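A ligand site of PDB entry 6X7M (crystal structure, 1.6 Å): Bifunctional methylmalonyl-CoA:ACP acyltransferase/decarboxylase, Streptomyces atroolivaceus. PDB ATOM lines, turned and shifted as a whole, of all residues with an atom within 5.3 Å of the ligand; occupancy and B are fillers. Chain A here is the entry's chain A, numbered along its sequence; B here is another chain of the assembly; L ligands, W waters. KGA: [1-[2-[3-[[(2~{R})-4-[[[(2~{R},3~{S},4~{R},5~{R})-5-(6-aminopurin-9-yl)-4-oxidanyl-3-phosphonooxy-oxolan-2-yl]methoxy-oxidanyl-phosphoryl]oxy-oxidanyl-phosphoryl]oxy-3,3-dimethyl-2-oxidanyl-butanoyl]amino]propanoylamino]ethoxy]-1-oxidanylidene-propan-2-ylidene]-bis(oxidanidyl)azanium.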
ATOM      1  N   TRP A  39      -8.315   7.774 -19.805  1.00  0.00           N
ATOM      2  CA  TRP A  39      -7.011   7.970 -19.144  1.00  0.00           C
ATOM      3  C   TRP A  39      -5.896   7.757 -20.173  1.00  0.00           C
ATOM      4  O   TRP A  39      -4.935   8.480 -20.039  1.00  0.00           O
ATOM      5  CB  TRP A  39      -6.849   7.101 -17.908  1.00  0.00           C
ATOM      6  CG  TRP A  39      -7.544   7.674 -16.708  1.00  0.00           C
ATOM      7  CD1 TRP A  39      -8.571   8.572 -16.684  1.00  0.00           C
ATOM      8  CD2 TRP A  39      -7.191   7.437 -15.339  1.00  0.00           C
ATOM      9  NE1 TRP A  39      -8.879   8.877 -15.387  1.00  0.00           N
ATOM     10  CE2 TRP A  39      -8.053   8.200 -14.536  1.00  0.00           C
ATOM     11  CE3 TRP A  39      -6.207   6.676 -14.701  1.00  0.00           C
ATOM     12  CZ2 TRP A  39      -7.961   8.237 -13.150  1.00  0.00           C
ATOM     13  CZ3 TRP A  39      -6.100   6.716 -13.331  1.00  0.00           C
ATOM     14  CH2 TRP A  39      -6.966   7.461 -12.553  1.00  0.00           C
ATOM     15  N   LEU A  63      -7.292  11.658 -11.879  1.00  0.00           N
ATOM     16  CA  LEU A  63      -8.073  12.381 -12.920  1.00  0.00           C
ATOM     17  C   LEU A  63      -9.528  11.942 -12.842  1.00  0.00           C
ATOM     18  O   LEU A  63      -9.991  11.077 -13.603  1.00  0.00           O
ATOM     19  CB  LEU A  63      -7.460  12.158 -14.299  1.00  0.00           C
ATOM     20  CG  LEU A  63      -8.147  12.975 -15.398  1.00  0.00           C
ATOM     21  CD1 LEU A  63      -8.296  14.458 -15.050  1.00  0.00           C
ATOM     22  CD2 LEU A  63      -7.482  12.802 -16.746  1.00  0.00           C
ATOM     23  N   ALA A  64     -10.209  12.427 -11.817  1.00  0.00           N
ATOM     24  CA  ALA A  64     -11.513  11.882 -11.375  1.00  0.00           C
ATOM     25  C   ALA A  64     -12.574  12.185 -12.428  1.00  0.00           C
ATOM     26  O   ALA A  64     -12.637  13.287 -12.964  1.00  0.00           O
ATOM     27  CB  ALA A  64     -11.902  12.505 -10.085  1.00  0.00           C
ATOM     28  N   PHE A  65     -13.481  11.220 -12.624  1.00  0.00           N
ATOM     29  CA  PHE A  65     -14.670  11.408 -13.474  1.00  0.00           C
ATOM     30  C   PHE A  65     -15.569  12.382 -12.765  1.00  0.00           C
ATOM     31  O   PHE A  65     -15.790  12.164 -11.531  1.00  0.00           O
ATOM     32  CB  PHE A  65     -15.302  10.044 -13.805  1.00  0.00           C
ATOM     33  CG  PHE A  65     -14.392   9.216 -14.709  1.00  0.00           C
ATOM     34  CD1 PHE A  65     -13.317   8.497 -14.199  1.00  0.00           C
ATOM     35  CD2 PHE A  65     -14.521   9.287 -16.090  1.00  0.00           C
ATOM     36  CE1 PHE A  65     -12.402   7.852 -15.025  1.00  0.00           C
ATOM     37  CE2 PHE A  65     -13.616   8.620 -16.910  1.00  0.00           C
ATOM     38  CZ  PHE A  65     -12.536   7.930 -16.384  1.00  0.00           C
ATOM     39  N   TYR A  66     -16.098  13.364 -13.481  1.00  0.00           N
ATOM     40  CA  TYR A  66     -16.993  14.382 -12.879  1.00  0.00           C
ATOM     41  C   TYR A  66     -18.320  14.450 -13.654  1.00  0.00           C
ATOM     42  O   TYR A  66     -19.373  14.489 -13.061  1.00  0.00           O
ATOM     43  CB  TYR A  66     -16.307  15.741 -12.806  1.00  0.00           C
ATOM     44  CG  TYR A  66     -17.179  16.714 -12.080  1.00  0.00           C
ATOM     45  CD1 TYR A  66     -17.287  16.658 -10.702  1.00  0.00           C
ATOM     46  CD2 TYR A  66     -18.000  17.573 -12.769  1.00  0.00           C
ATOM     47  CE1 TYR A  66     -18.154  17.485 -10.016  1.00  0.00           C
ATOM     48  CE2 TYR A  66     -18.886  18.400 -12.088  1.00  0.00           C
ATOM     49  CZ  TYR A  66     -18.972  18.336 -10.716  1.00  0.00           C
ATOM     50  OH  TYR A  66     -19.850  19.188 -10.071  1.00  0.00           O
ATOM     51  N   ARG A 140     -11.667  15.843 -13.600  1.00  0.00           N
ATOM     52  CA  ARG A 140     -11.055  16.921 -12.763  1.00  0.00           C
ATOM     53  C   ARG A 140      -9.962  16.273 -11.917  1.00  0.00           C
ATOM     54  O   ARG A 140     -10.246  15.292 -11.240  1.00  0.00           O
ATOM     55  CB  ARG A 140     -12.130  17.527 -11.867  1.00  0.00           C
ATOM     56  CG  ARG A 140     -13.260  18.165 -12.651  1.00  0.00           C
ATOM     57  CD  ARG A 140     -14.390  18.616 -11.759  1.00  0.00           C
ATOM     58  NE  ARG A 140     -14.093  19.918 -11.185  1.00  0.00           N
ATOM     59  CZ  ARG A 140     -15.006  20.730 -10.647  1.00  0.00           C
ATOM     60  NH1 ARG A 140     -16.282  20.408 -10.603  1.00  0.00           N
ATOM     61  NH2 ARG A 140     -14.609  21.873 -10.122  1.00  0.00           N
ATOM     62  N   VAL A 142      -7.910  15.634  -8.755  1.00  0.00           N
ATOM     63  CA  VAL A 142      -8.165  15.782  -7.311  1.00  0.00           C
ATOM     64  C   VAL A 142      -7.080  15.068  -6.507  1.00  0.00           C
ATOM     65  O   VAL A 142      -6.479  14.120  -7.014  1.00  0.00           O
ATOM     66  CB  VAL A 142      -9.570  15.278  -6.929  1.00  0.00           C
ATOM     67  CG1 VAL A 142     -10.655  16.028  -7.697  1.00  0.00           C
ATOM     68  CG2 VAL A 142      -9.676  13.800  -7.119  1.00  0.00           C
ATOM     69  N   LEU A 153     -12.482  16.085  -1.205  1.00  0.00           N
ATOM     70  CA  LEU A 153     -11.335  16.013  -2.134  1.00  0.00           C
ATOM     71  C   LEU A 153     -11.024  17.445  -2.607  1.00  0.00           C
ATOM     72  O   LEU A 153     -11.928  18.321  -2.577  1.00  0.00           O
ATOM     73  CB  LEU A 153     -11.698  15.082  -3.295  1.00  0.00           C
ATOM     74  CG  LEU A 153     -12.119  13.655  -2.920  1.00  0.00           C
ATOM     75  CD1 LEU A 153     -12.489  12.860  -4.199  1.00  0.00           C
ATOM     76  CD2 LEU A 153     -11.044  12.914  -2.153  1.00  0.00           C
ATOM     77  N   VAL A 154      -9.767  17.649  -2.931  1.00  0.00           N
ATOM     78  CA  VAL A 154      -9.141  18.971  -3.240  1.00  0.00           C
ATOM     79  C   VAL A 154      -8.724  19.017  -4.701  1.00  0.00           C
ATOM     80  O   VAL A 154      -8.091  18.052  -5.213  1.00  0.00           O
ATOM     81  CB  VAL A 154      -7.933  19.189  -2.318  1.00  0.00           C
ATOM     82  CG1 VAL A 154      -7.375  20.595  -2.445  1.00  0.00           C
ATOM     83  CG2 VAL A 154      -8.264  18.868  -0.875  1.00  0.00           C
ATOM     84  N   LYS A 155      -8.993  20.132  -5.367  1.00  0.00           N
ATOM     85  CA  LYS A 155      -8.591  20.303  -6.783  1.00  0.00           C
ATOM     86  C   LYS A 155      -7.063  20.284  -6.876  1.00  0.00           C
ATOM     87  O   LYS A 155      -6.326  20.647  -5.902  1.00  0.00           O
ATOM     88  CB  LYS A 155      -9.186  21.587  -7.359  1.00  0.00           C
ATOM     89  CG  LYS A 155      -8.616  22.869  -6.805  1.00  0.00           C
ATOM     90  CD  LYS A 155      -9.417  24.108  -7.208  1.00  0.00           C
ATOM     91  CE  LYS A 155      -8.780  24.894  -8.326  1.00  0.00           C
ATOM     92  NZ  LYS A 155      -7.691  25.760  -7.809  1.00  0.00           N
ATOM     93  N   ARG A 183     -26.958  19.653 -10.941  1.00  0.00           N
ATOM     94  CA  ARG A 183     -26.790  19.552  -9.462  1.00  0.00           C
ATOM     95  C   ARG A 183     -27.902  20.333  -8.779  1.00  0.00           C
ATOM     96  O   ARG A 183     -28.260  19.993  -7.604  1.00  0.00           O
ATOM     97  CB  ARG A 183     -25.487  20.160  -8.941  1.00  0.00           C
ATOM     98  CG  ARG A 183     -24.295  19.733  -9.752  1.00  0.00           C
ATOM     99  CD  ARG A 183     -23.027  20.397  -9.221  1.00  0.00           C
ATOM    100  NE  ARG A 183     -22.919  21.836  -9.368  1.00  0.00           N
ATOM    101  CZ  ARG A 183     -21.773  22.501  -9.561  1.00  0.00           C
ATOM    102  NH1 ARG A 183     -21.779  23.824  -9.648  1.00  0.00           N
ATOM    103  NH2 ARG A 183     -20.611  21.870  -9.713  1.00  0.00           N
ATOM    104  N   ASN A 216     -12.337   0.988  -5.859  1.00  0.00           N
ATOM    105  CA  ASN A 216     -11.262   0.973  -6.880  1.00  0.00           C
ATOM    106  C   ASN A 216      -9.878   0.763  -6.235  1.00  0.00           C
ATOM    107  O   ASN A 216      -9.748   0.559  -5.008  1.00  0.00           O
ATOM    108  CB  ASN A 216     -11.377   2.207  -7.773  1.00  0.00           C
ATOM    109  CG  ASN A 216     -10.896   3.484  -7.148  1.00  0.00           C
ATOM    110  OD1 ASN A 216     -10.247   3.467  -6.092  1.00  0.00           O
ATOM    111  ND2 ASN A 216     -11.204   4.612  -7.780  1.00  0.00           N
ATOM    112  N   LEU A 220     -11.125   4.522  -3.415  1.00  0.00           N
ATOM    113  CA  LEU A 220     -12.324   5.375  -3.605  1.00  0.00           C
ATOM    114  C   LEU A 220     -13.489   4.512  -4.108  1.00  0.00           C
ATOM    115  O   LEU A 220     -13.223   3.411  -4.613  1.00  0.00           O
ATOM    116  CB  LEU A 220     -12.051   6.469  -4.632  1.00  0.00           C
ATOM    117  CG  LEU A 220     -11.008   7.511  -4.247  1.00  0.00           C
ATOM    118  CD1 LEU A 220     -10.547   8.274  -5.442  1.00  0.00           C
ATOM    119  CD2 LEU A 220     -11.582   8.446  -3.217  1.00  0.00           C
ATOM    120  N   LEU A 221     -14.711   5.049  -4.118  1.00  0.00           N
ATOM    121  CA  LEU A 221     -15.805   4.360  -4.850  1.00  0.00           C
ATOM    122  C   LEU A 221     -15.439   4.485  -6.322  1.00  0.00           C
ATOM    123  O   LEU A 221     -15.083   5.604  -6.765  1.00  0.00           O
ATOM    124  CB  LEU A 221     -17.124   5.092  -4.617  1.00  0.00           C
ATOM    125  CG  LEU A 221     -17.674   5.063  -3.207  1.00  0.00           C
ATOM    126  CD1 LEU A 221     -19.059   5.672  -3.236  1.00  0.00           C
ATOM    127  CD2 LEU A 221     -17.726   3.639  -2.660  1.00  0.00           C
ATOM    128  N   TYR A 222     -15.524   3.376  -7.036  1.00  0.00           N
ATOM    129  CA  TYR A 222     -15.118   3.267  -8.469  1.00  0.00           C
ATOM    130  C   TYR A 222     -16.132   4.007  -9.356  1.00  0.00           C
ATOM    131  O   TYR A 222     -17.361   3.809  -9.232  1.00  0.00           O
ATOM    132  CB  TYR A 222     -15.115   1.780  -8.852  1.00  0.00           C
ATOM    133  CG  TYR A 222     -14.698   1.394 -10.249  1.00  0.00           C
ATOM    134  CD1 TYR A 222     -13.643   2.020 -10.905  1.00  0.00           C
ATOM    135  CD2 TYR A 222     -15.341   0.318 -10.874  1.00  0.00           C
ATOM    136  CE1 TYR A 222     -13.218   1.566 -12.153  1.00  0.00           C
ATOM    137  CE2 TYR A 222     -14.910  -0.148 -12.102  1.00  0.00           C
ATOM    138  CZ  TYR A 222     -13.879   0.506 -12.750  1.00  0.00           C
ATOM    139  OH  TYR A 222     -13.538   0.025 -13.991  1.00  0.00           O
ATOM    140  N   PHE A 223     -15.644   4.801 -10.291  1.00  0.00           N
ATOM    141  CA  PHE A 223     -16.553   5.631 -11.119  1.00  0.00           C
ATOM    142  C   PHE A 223     -17.594   4.725 -11.785  1.00  0.00           C
ATOM    143  O   PHE A 223     -18.794   5.120 -11.945  1.00  0.00           O
ATOM    144  CB  PHE A 223     -15.806   6.484 -12.150  1.00  0.00           C
ATOM    145  CG  PHE A 223     -15.273   5.716 -13.333  1.00  0.00           C
ATOM    146  CD1 PHE A 223     -14.083   5.038 -13.256  1.00  0.00           C
ATOM    147  CD2 PHE A 223     -15.975   5.647 -14.538  1.00  0.00           C
ATOM    148  CE1 PHE A 223     -13.598   4.314 -14.331  1.00  0.00           C
ATOM    149  CE2 PHE A 223     -15.513   4.900 -15.600  1.00  0.00           C
ATOM    150  CZ  PHE A 223     -14.306   4.252 -15.515  1.00  0.00           C
ATOM    151  N   ALA A 224     -17.235   3.521 -12.231  1.00  0.00           N
ATOM    152  CA  ALA A 224     -18.191   2.685 -13.002  1.00  0.00           C
ATOM    153  C   ALA A 224     -19.263   2.142 -12.037  1.00  0.00           C
ATOM    154  O   ALA A 224     -20.383   1.818 -12.465  1.00  0.00           O
ATOM    155  CB  ALA A 224     -17.504   1.597 -13.798  1.00  0.00           C
ATOM    156  N   TYR A 226     -20.853   3.762  -9.899  1.00  0.00           N
ATOM    157  CA  TYR A 226     -21.946   4.746  -9.785  1.00  0.00           C
ATOM    158  C   TYR A 226     -23.020   4.388 -10.818  1.00  0.00           C
ATOM    159  O   TYR A 226     -24.209   4.480 -10.561  1.00  0.00           O
ATOM    160  CB  TYR A 226     -21.480   6.172  -9.962  1.00  0.00           C
ATOM    161  CG  TYR A 226     -20.759   6.781  -8.791  1.00  0.00           C
ATOM    162  CD1 TYR A 226     -19.503   6.345  -8.427  1.00  0.00           C
ATOM    163  CD2 TYR A 226     -21.245   7.912  -8.148  1.00  0.00           C
ATOM    164  CE1 TYR A 226     -18.768   6.968  -7.437  1.00  0.00           C
ATOM    165  CE2 TYR A 226     -20.522   8.543  -7.150  1.00  0.00           C
ATOM    166  CZ  TYR A 226     -19.292   8.051  -6.758  1.00  0.00           C
ATOM    167  OH  TYR A 226     -18.556   8.721  -5.824  1.00  0.00           O
ATOM    168  N   TYR A 260     -20.774  13.261 -10.901  1.00  0.00           N
ATOM    169  CA  TYR A 260     -20.111  12.743  -9.704  1.00  0.00           C
ATOM    170  C   TYR A 260     -19.783  13.932  -8.775  1.00  0.00           C
ATOM    171  O   TYR A 260     -18.711  14.555  -8.825  1.00  0.00           O
ATOM    172  CB  TYR A 260     -18.819  12.016 -10.077  1.00  0.00           C
ATOM    173  CG  TYR A 260     -18.939  10.816 -10.968  1.00  0.00           C
ATOM    174  CD1 TYR A 260     -18.957  10.935 -12.346  1.00  0.00           C
ATOM    175  CD2 TYR A 260     -19.015   9.542 -10.427  1.00  0.00           C
ATOM    176  CE1 TYR A 260     -19.007   9.820 -13.157  1.00  0.00           C
ATOM    177  CE2 TYR A 260     -19.048   8.427 -11.224  1.00  0.00           C
ATOM    178  CZ  TYR A 260     -19.059   8.555 -12.588  1.00  0.00           C
ATOM    179  OH  TYR A 260     -19.092   7.465 -13.433  1.00  0.00           O
ATOM    180  N   LEU A 261     -20.701  14.257  -7.891  1.00  0.00           N
ATOM    181  CA  LEU A 261     -20.606  15.433  -6.978  1.00  0.00           C
ATOM    182  C   LEU A 261     -19.704  15.122  -5.777  1.00  0.00           C
ATOM    183  O   LEU A 261     -19.138  16.078  -5.197  1.00  0.00           O
ATOM    184  CB  LEU A 261     -22.005  15.847  -6.498  1.00  0.00           C
ATOM    185  CG  LEU A 261     -22.953  16.532  -7.480  1.00  0.00           C
ATOM    186  CD1 LEU A 261     -22.207  17.195  -8.610  1.00  0.00           C
ATOM    187  CD2 LEU A 261     -24.003  15.590  -8.019  1.00  0.00           C
ATOM    188  N   GLY A 262     -19.601  13.858  -5.379  1.00  0.00           N
ATOM    189  CA  GLY A 262     -18.738  13.443  -4.255  1.00  0.00           C
ATOM    190  C   GLY A 262     -18.412  11.973  -4.361  1.00  0.00           C
ATOM    191  O   GLY A 262     -19.088  11.234  -5.114  1.00  0.00           O
ATOM    192  N   ASN A 263     -17.396  11.564  -3.614  1.00  0.00           N
ATOM    193  CA  ASN A 263     -17.062  10.170  -3.345  1.00  0.00           C
ATOM    194  C   ASN A 263     -17.582   9.880  -1.932  1.00  0.00           C
ATOM    195  O   ASN A 263     -18.260  10.743  -1.352  1.00  0.00           O
ATOM    196  CB  ASN A 263     -15.562   9.909  -3.541  1.00  0.00           C
ATOM    197  CG  ASN A 263     -15.316   8.488  -4.001  1.00  0.00           C
ATOM    198  OD1 ASN A 263     -15.267   7.572  -3.183  1.00  0.00           O
ATOM    199  ND2 ASN A 263     -15.164   8.286  -5.311  1.00  0.00           N
ATOM    200  N   PRO B  21      -7.440   1.761 -13.824  1.00  0.00           N
ATOM    201  CA  PRO B  21      -8.590   1.553 -12.925  1.00  0.00           C
ATOM    202  C   PRO B  21      -9.441   0.311 -13.219  1.00  0.00           C
ATOM    203  O   PRO B  21     -10.007  -0.269 -12.335  1.00  0.00           O
ATOM    204  CB  PRO B  21      -9.378   2.839 -13.131  1.00  0.00           C
ATOM    205  CG  PRO B  21      -8.348   3.882 -13.497  1.00  0.00           C
ATOM    206  CD  PRO B  21      -7.342   3.144 -14.344  1.00  0.00           C
ATOM    207  N   PHE B  83      -3.001   2.016  -9.352  1.00  0.00           N
ATOM    208  CA  PHE B  83      -2.967   2.837 -10.579  1.00  0.00           C
ATOM    209  C   PHE B  83      -1.521   3.235 -10.904  1.00  0.00           C
ATOM    210  O   PHE B  83      -0.845   3.743  -9.996  1.00  0.00           O
ATOM    211  CB  PHE B  83      -3.820   4.080 -10.392  1.00  0.00           C
ATOM    212  CG  PHE B  83      -5.298   3.889 -10.129  1.00  0.00           C
ATOM    213  CD1 PHE B  83      -5.883   2.628 -10.124  1.00  0.00           C
ATOM    214  CD2 PHE B  83      -6.076   4.995  -9.933  1.00  0.00           C
ATOM    215  CE1 PHE B  83      -7.260   2.515  -9.867  1.00  0.00           C
ATOM    216  CE2 PHE B  83      -7.439   4.885  -9.694  1.00  0.00           C
ATOM    217  CZ  PHE B  83      -8.015   3.649  -9.641  1.00  0.00           C
HETATM  218  O5' KGA L   1     -13.588  22.864  -5.257  1.00  0.00           O
HETATM  219  P1  KGA L   1     -15.147  23.010  -5.309  1.00  0.00           P
HETATM  220  O11 KGA L   1     -15.600  24.387  -5.174  1.00  0.00           O
HETATM  221  O12 KGA L   1     -15.654  22.506  -6.570  1.00  0.00           O
HETATM  222  O6  KGA L   1     -15.696  22.006  -4.262  1.00  0.00           O
HETATM  223  P2  KGA L   1     -16.481  20.741  -4.741  1.00  0.00           P
HETATM  224  O21 KGA L   1     -17.142  20.321  -3.495  1.00  0.00           O
HETATM  225  O22 KGA L   1     -17.476  20.916  -5.795  1.00  0.00           O
HETATM  226  O7  KGA L   1     -15.491  19.602  -5.213  1.00  0.00           O
HETATM  227  CPB KGA L   1     -15.243  19.280  -6.558  1.00  0.00           C
HETATM  228  CPA KGA L   1     -14.873  17.809  -6.549  1.00  0.00           C
HETATM  229  CP9 KGA L   1     -13.727  17.586  -5.600  1.00  0.00           C
HETATM  230  CP8 KGA L   1     -14.428  17.413  -7.930  1.00  0.00           C
HETATM  231  CP7 KGA L   1     -16.072  17.005  -6.077  1.00  0.00           C
HETATM  232  OP3 KGA L   1     -17.168  17.318  -6.908  1.00  0.00           O
HETATM  233  CP6 KGA L   1     -15.808  15.525  -6.054  1.00  0.00           C
HETATM  234  OP2 KGA L   1     -15.141  15.041  -5.215  1.00  0.00           O
HETATM  235  NP2 KGA L   1     -16.381  14.813  -6.976  1.00  0.00           N
HETATM  236  CP5 KGA L   1     -16.433  13.432  -6.859  1.00  0.00           C
HETATM  237  CP4 KGA L   1     -15.564  12.638  -7.892  1.00  0.00           C
HETATM  238  CP3 KGA L   1     -15.431  11.105  -8.002  1.00  0.00           C
HETATM  239  OP1 KGA L   1     -15.299  10.560  -6.946  1.00  0.00           O
HETATM  240  NP1 KGA L   1     -15.536  10.537  -9.175  1.00  0.00           N
HETATM  241  CP2 KGA L   1     -15.508   9.093  -9.245  1.00  0.00           C
HETATM  242  CP1 KGA L   1     -14.268   8.610  -8.517  1.00  0.00           C
HETATM  243  O   KGA L   1     -13.617   7.666  -9.271  1.00  0.00           O
HETATM  244  CS1 KGA L   1     -12.766   8.008 -10.358  1.00  0.00           C
HETATM  245  OS1 KGA L   1     -12.837   9.090 -10.816  1.00  0.00           O
HETATM  246  CS2 KGA L   1     -11.832   6.987 -10.910  1.00  0.00           C
HETATM  247  CS3 KGA L   1     -10.710   7.425 -11.815  1.00  0.00           C
HETATM  248  NS4 KGA L   1     -11.987   5.572 -10.573  1.00  0.00           N
HETATM  249  OS5 KGA L   1     -11.186   4.763 -11.034  1.00  0.00           O
HETATM  250  OS4 KGA L   1     -12.891   5.170  -9.850  1.00  0.00           O
HETATM  251  O   HOH W   1     -10.673  22.208  -4.193  1.00  0.00           O
HETATM  252  O   HOH W   2     -15.161  15.693  -2.576  1.00  0.00           O
HETATM  253  O   HOH W   3     -19.857  18.919  -6.675  1.00  0.00           O
HETATM  254  O   HOH W   4     -13.189  22.009  -7.605  1.00  0.00           O
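OS4 of the ligand lies within hydrogen-bond range of ND2 of Asn 216, 2.7 Å away.
ND2 of Asn 263 is in hydrogen-bond range of OP1 of the ligand, at 2.8 Å.
The backbone NH (N) of Phe 223 sits at hydrogen-bond distance from an oxygen (OS4) of the ligand (2.8 Å).
The backbone NH (N) of Phe 65 is in hydrogen-bond range of an oxygen (OS1) of the ligand, 2.9 Å away.
The backbone carbonyl oxygen (O) of Phe 65 lies within hydrogen-bond range of a nitrogen (NP1) of the ligand, at 2.9 Å.
O of Leu 261 lies within hydrogen-bond range of OP3 of the ligand, at 2.9 Å.
NP2 of the ligand lies within hydrogen-bond range of O of Tyr 260 (3.0 Å).
The guanidinium group (NH2) of Arg 140 lies within salt-bridge range of an oxygen (O12) of the ligand (3.8 Å).
The backbone NH of Leu 220 sits at hydrogen-bond distance from the side-chain amide oxygen of Asn 216, at 3.0 Å.
The backbone NH (N) of Leu 221 is in hydrogen-bond range of the side-chain amide oxygen (OD1) of Asn 263 (2.7 Å).
The side-chain hydroxyl (OH) of Tyr 260 sits at hydrogen-bond distance from the backbone carbonyl oxygen (O) of Phe 223 (2.8 Å).
The backbone carbonyl oxygen (O) of Tyr 66 is in hydrogen-bond range of the backbone NH (N) of Tyr 260.
N of Arg 140 sits at hydrogen-bond distance from O of Ala 64.
The indole nitrogen (NE1) of Trp 39 is in hydrogen-bond range of the backbone carbonyl oxygen (O) of Leu 63 (3.0 Å).
OH of Tyr 66 is in hydrogen-bond range of NH2 of Arg 183, at 2.8 Å.
The backbone carbonyl oxygen (O) of Gly 262 is in hydrogen-bond range of the side-chain hydroxyl (OH) of Tyr 226 (2.7 Å).
CZ2 of Trp 39 touches CS3 of the ligand (3.2 Å).
Ala 64 touches the ligand (CA to OS1, 3.1 Å).
Tyr 66 touches the ligand (CE1 to OP3, 3.3 Å).
Leu 153 touches the ligand.
Leu 221 touches the ligand.
CA of Tyr 222 touches OS4 of the ligand, at 3.2 Å.
OH of Tyr 226 touches OP1 of the ligand (3.9 Å).
CA of Gly 262 touches CP5 of the ligand, at 3.5 Å.
Pro 21 of chain B touches the ligand.
CZ of Phe 83 of chain B touches OS5 of the ligand, at 3.6 Å.
Hydrophobic or aromatic side chains that line the ligand: Trp 39, Ala 64, Phe 65, Tyr 66, Leu 153, Tyr 222, Phe 223, Tyr 260, Pro 21 of chain B and Phe 83 of chain B.
Water W4 lies within hydrogen-bond range of O5' of the ligand and NH2 of Arg 140.
Water W2 lies within hydrogen-bond range of an oxygen (OP2) of the ligand (2.7 Å) and the backbone NH (N) of Leu 153 (3.0 Å).
Water W3 lies within hydrogen-bond range of OP3 of the ligand (3.1 Å), O of Leu 261 (3.3 Å) and OH of Tyr 66 (3.4 Å).
Water W1 bridges N of Lys 155 (2.9 Å) and O5' of the ligand (3.2 Å).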
